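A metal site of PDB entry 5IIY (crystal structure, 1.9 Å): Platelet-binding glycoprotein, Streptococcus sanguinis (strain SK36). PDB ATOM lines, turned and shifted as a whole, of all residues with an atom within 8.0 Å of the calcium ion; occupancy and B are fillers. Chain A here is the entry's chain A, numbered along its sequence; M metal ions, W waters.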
ATOM      1  N   ALA A 122     -17.049  -2.052  -7.363  1.00  0.00           N
ATOM      2  CA  ALA A 122     -15.771  -2.756  -7.331  1.00  0.00           C
ATOM      3  C   ALA A 122     -14.930  -2.250  -6.172  1.00  0.00           C
ATOM      4  O   ALA A 122     -15.026  -1.091  -5.776  1.00  0.00           O
ATOM      5  CB  ALA A 122     -15.036  -2.579  -8.646  1.00  0.00           C
ATOM      6  N   GLN A 123     -14.090  -3.129  -5.624  1.00  0.00           N
ATOM      7  CA  GLN A 123     -13.298  -2.790  -4.454  1.00  0.00           C
ATOM      8  C   GLN A 123     -12.357  -1.601  -4.671  1.00  0.00           C
ATOM      9  O   GLN A 123     -12.011  -0.913  -3.719  1.00  0.00           O
ATOM     10  CB  GLN A 123     -12.480  -3.998  -3.996  1.00  0.00           C
ATOM     11  CG  GLN A 123     -13.266  -4.940  -3.106  1.00  0.00           C
ATOM     12  CD  GLN A 123     -12.477  -6.154  -2.725  1.00  0.00           C
ATOM     13  OE1 GLN A 123     -12.186  -7.012  -3.555  1.00  0.00           O
ATOM     14  NE2 GLN A 123     -12.111  -6.254  -1.459  1.00  0.00           N
ATOM     15  N   THR A 124     -11.930  -1.352  -5.908  1.00  0.00           N
ATOM     16  CA  THR A 124     -10.997  -0.243  -6.092  1.00  0.00           C
ATOM     17  C   THR A 124     -11.709   1.088  -5.929  1.00  0.00           C
ATOM     18  O   THR A 124     -11.066   2.126  -5.793  1.00  0.00           O
ATOM     19  CB  THR A 124     -10.283  -0.278  -7.464  1.00  0.00           C
ATOM     20  OG1 THR A 124      -9.371   0.829  -7.538  1.00  0.00           O
ATOM     21  CG2 THR A 124     -11.281  -0.195  -8.605  1.00  0.00           C
ATOM     22  N   ASP A 125     -13.042   1.073  -5.913  1.00  0.00           N
ATOM     23  CA  ASP A 125     -13.788   2.300  -5.664  1.00  0.00           C
ATOM     24  C   ASP A 125     -13.658   2.712  -4.206  1.00  0.00           C
ATOM     25  O   ASP A 125     -13.710   3.899  -3.880  1.00  0.00           O
ATOM     26  CB  ASP A 125     -15.261   2.120  -6.049  1.00  0.00           C
ATOM     27  CG  ASP A 125     -15.482   2.117  -7.551  1.00  0.00           C
ATOM     28  OD1 ASP A 125     -14.470   2.101  -8.283  1.00  0.00           O
ATOM     29  OD2 ASP A 125     -16.647   2.127  -7.986  1.00  0.00           O
ATOM     30  N   LYS A 126     -13.480   1.734  -3.328  1.00  0.00           N
ATOM     31  CA  LYS A 126     -13.329   2.024  -1.896  1.00  0.00           C
ATOM     32  C   LYS A 126     -11.901   2.415  -1.534  1.00  0.00           C
ATOM     33  O   LYS A 126     -11.670   3.214  -0.619  1.00  0.00           O
ATOM     34  CB  LYS A 126     -13.761   0.813  -1.063  1.00  0.00           C
ATOM     35  CG  LYS A 126     -13.583   1.003   0.431  1.00  0.00           C
ATOM     36  CD  LYS A 126     -14.014  -0.222   1.205  1.00  0.00           C
ATOM     37  CE  LYS A 126     -13.660  -0.082   2.676  1.00  0.00           C
ATOM     38  NZ  LYS A 126     -14.081  -1.269   3.458  1.00  0.00           N
ATOM     39  N   TYR A 127     -10.930   1.864  -2.268  1.00  0.00           N
ATOM     40  CA  TYR A 127      -9.536   2.032  -1.884  1.00  0.00           C
ATOM     41  C   TYR A 127      -8.770   2.980  -2.803  1.00  0.00           C
ATOM     42  O   TYR A 127      -8.866   2.916  -4.041  1.00  0.00           O
ATOM     43  CB  TYR A 127      -8.853   0.666  -1.831  1.00  0.00           C
ATOM     44  CG  TYR A 127      -9.517  -0.244  -0.838  1.00  0.00           C
ATOM     45  CD1 TYR A 127      -9.364  -0.043   0.532  1.00  0.00           C
ATOM     46  CD2 TYR A 127     -10.312  -1.307  -1.253  1.00  0.00           C
ATOM     47  CE1 TYR A 127      -9.970  -0.868   1.450  1.00  0.00           C
ATOM     48  CE2 TYR A 127     -10.919  -2.148  -0.341  1.00  0.00           C
ATOM     49  CZ  TYR A 127     -10.749  -1.915   1.007  1.00  0.00           C
ATOM     50  OH  TYR A 127     -11.365  -2.750   1.918  1.00  0.00           O
ATOM     51  N   ASN A 128      -8.009   3.859  -2.155  1.00  0.00           N
ATOM     52  CA  ASN A 128      -7.166   4.825  -2.841  1.00  0.00           C
ATOM     53  C   ASN A 128      -5.753   4.746  -2.282  1.00  0.00           C
ATOM     54  O   ASN A 128      -5.485   5.286  -1.213  1.00  0.00           O
ATOM     55  CB  ASN A 128      -7.726   6.242  -2.680  1.00  0.00           C
ATOM     56  CG  ASN A 128      -7.279   7.168  -3.780  1.00  0.00           C
ATOM     57  OD1 ASN A 128      -7.874   7.197  -4.854  1.00  0.00           O
ATOM     58  ND2 ASN A 128      -6.223   7.946  -3.525  1.00  0.00           N
ATOM     59  N   PRO A 129      -4.859   4.058  -2.996  1.00  0.00           N
ATOM     60  CA  PRO A 129      -3.519   3.757  -2.469  1.00  0.00           C
ATOM     61  C   PRO A 129      -2.615   4.979  -2.339  1.00  0.00           C
ATOM     62  O   PRO A 129      -2.503   5.779  -3.274  1.00  0.00           O
ATOM     63  CB  PRO A 129      -2.951   2.774  -3.492  1.00  0.00           C
ATOM     64  CG  PRO A 129      -3.677   3.092  -4.761  1.00  0.00           C
ATOM     65  CD  PRO A 129      -5.066   3.497  -4.336  1.00  0.00           C
ATOM     66  N   ILE A 162      -5.573  -1.085   3.122  1.00  0.00           N
ATOM     67  CA  ILE A 162      -5.896  -1.931   1.974  1.00  0.00           C
ATOM     68  C   ILE A 162      -6.003  -3.382   2.433  1.00  0.00           C
ATOM     69  O   ILE A 162      -5.326  -3.764   3.392  1.00  0.00           O
ATOM     70  CB  ILE A 162      -4.831  -1.750   0.854  1.00  0.00           C
ATOM     71  CG1 ILE A 162      -5.406  -0.908  -0.297  1.00  0.00           C
ATOM     72  CG2 ILE A 162      -4.282  -3.077   0.355  1.00  0.00           C
ATOM     73  CD1 ILE A 162      -4.365  -0.517  -1.330  1.00  0.00           C
ATOM     74  N   ILE A 178      -1.980  -3.130  -7.892  1.00  0.00           N
ATOM     75  CA  ILE A 178      -2.678  -3.650  -6.729  1.00  0.00           C
ATOM     76  C   ILE A 178      -3.964  -4.316  -7.196  1.00  0.00           C
ATOM     77  O   ILE A 178      -4.878  -3.642  -7.675  1.00  0.00           O
ATOM     78  CB  ILE A 178      -3.001  -2.543  -5.714  1.00  0.00           C
ATOM     79  CG1 ILE A 178      -1.724  -1.829  -5.257  1.00  0.00           C
ATOM     80  CG2 ILE A 178      -3.763  -3.128  -4.510  1.00  0.00           C
ATOM     81  CD1 ILE A 178      -1.983  -0.617  -4.389  1.00  0.00           C
ATOM     82  N   TYR A 180      -7.182  -6.107  -6.089  1.00  0.00           N
ATOM     83  CA  TYR A 180      -8.032  -6.367  -4.940  1.00  0.00           C
ATOM     84  C   TYR A 180      -8.688  -7.749  -5.049  1.00  0.00           C
ATOM     85  O   TYR A 180      -8.702  -8.343  -6.114  1.00  0.00           O
ATOM     86  CB  TYR A 180      -9.085  -5.248  -4.810  1.00  0.00           C
ATOM     87  CG  TYR A 180      -8.436  -3.900  -4.628  1.00  0.00           C
ATOM     88  CD1 TYR A 180      -7.935  -3.514  -3.399  1.00  0.00           C
ATOM     89  CD2 TYR A 180      -8.300  -3.021  -5.694  1.00  0.00           C
ATOM     90  CE1 TYR A 180      -7.326  -2.294  -3.229  1.00  0.00           C
ATOM     91  CE2 TYR A 180      -7.693  -1.790  -5.536  1.00  0.00           C
ATOM     92  CZ  TYR A 180      -7.205  -1.432  -4.297  1.00  0.00           C
ATOM     93  OH  TYR A 180      -6.605  -0.208  -4.137  1.00  0.00           O
ATOM     94  N   SER A 184     -10.597  -6.215  -9.261  1.00  0.00           N
ATOM     95  CA  SER A 184     -10.486  -4.817  -9.697  1.00  0.00           C
ATOM     96  C   SER A 184      -9.115  -4.324  -9.265  1.00  0.00           C
ATOM     97  O   SER A 184      -8.481  -4.941  -8.395  1.00  0.00           O
ATOM     98  CB  SER A 184     -11.608  -3.953  -9.118  1.00  0.00           C
ATOM     99  OG  SER A 184     -11.458  -3.768  -7.722  1.00  0.00           O
ATOM    100  N   THR A 185      -8.620  -3.240  -9.858  1.00  0.00           N
ATOM    101  CA  THR A 185      -7.233  -2.854  -9.623  1.00  0.00           C
ATOM    102  C   THR A 185      -6.979  -1.364  -9.364  1.00  0.00           C
ATOM    103  O   THR A 185      -7.836  -0.519  -9.605  1.00  0.00           O
ATOM    104  CB  THR A 185      -6.329  -3.247 -10.826  1.00  0.00           C
ATOM    105  OG1 THR A 185      -6.741  -2.526 -11.990  1.00  0.00           O
ATOM    106  CG2 THR A 185      -6.390  -4.738 -11.093  1.00  0.00           C
ATOM    107  N   ASP A 186      -5.786  -1.083  -8.873  1.00  0.00           N
ATOM    108  CA  ASP A 186      -5.218   0.262  -8.842  1.00  0.00           C
ATOM    109  C   ASP A 186      -3.790   0.139  -9.370  1.00  0.00           C
ATOM    110  O   ASP A 186      -3.153  -0.894  -9.173  1.00  0.00           O
ATOM    111  CB  ASP A 186      -5.249   0.866  -7.433  1.00  0.00           C
ATOM    112  CG  ASP A 186      -6.603   1.493  -7.061  1.00  0.00           C
ATOM    113  OD1 ASP A 186      -7.256   2.106  -7.915  1.00  0.00           O
ATOM    114  OD2 ASP A 186      -7.023   1.364  -5.898  1.00  0.00           O
ATOM    115  N   THR A 187      -3.308   1.161 -10.059  1.00  0.00           N
ATOM    116  CA  THR A 187      -1.957   1.160 -10.613  1.00  0.00           C
ATOM    117  C   THR A 187      -1.168   2.324 -10.023  1.00  0.00           C
ATOM    118  O   THR A 187      -1.727   3.398  -9.805  1.00  0.00           O
ATOM    119  CB  THR A 187      -1.978   1.276 -12.166  1.00  0.00           C
ATOM    120  OG1 THR A 187      -2.645   0.153 -12.728  1.00  0.00           O
ATOM    121  CG2 THR A 187      -0.555   1.347 -12.732  1.00  0.00           C
HETATM  122 CA    CA M   1      -8.860   2.800  -6.297  1.00  0.00          CA
HETATM  123  O   HOH W   1      -7.290   4.879  -6.411  1.00  0.00           O
HETATM  124  O   HOH W   2     -10.339   4.971  -5.265  1.00  0.00           O
HETATM  125  O   HOH W   3      -9.448   3.213  -8.378  1.00  0.00           O
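Water W3 is bound to the calcium ion (2.2 Å). O of Tyr 127 is bound to the calcium ion, 2.3 Å away. The backbone carbonyl oxygen (O) of Thr 124 is bound to the calcium ion (2.4 Å). The side-chain carboxylate (OD2) of Asp 186 binds the calcium ion (2.4 Å). The calcium ion is bound by OD1 of Asp 186 (2.4 Å). The side-chain hydroxyl (OG1) of Thr 124 is bound to the calcium ion (2.4 Å). The calcium ion is bound by water W1 (2.6 Å). Water W2 is bound to the calcium ion (2.8 Å).
The side-chain amino group of Lys 126 is in hydrogen-bond range of the side-chain hydroxyl of Tyr 127, 3.5 Å away. The side-chain hydroxyl (OG1) of Thr 124 sits close to the backbone carbonyl oxygen (O) of Thr 185 (2.9 Å). The backbone NH of Thr 124 is in hydrogen-bond range of the side-chain hydroxyl of Ser 184. The backbone NH (N) of Ile 178 is in hydrogen-bond range of the backbone carbonyl oxygen (O) of Asp 186, at 2.8 Å.
Three residues have an atom within 4 Å of the calcium ion: Thr 124, Tyr 127 and Asp 186. The nearest printed residue that does not touch the calcium ion is Pro 129 (4.3 Å).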
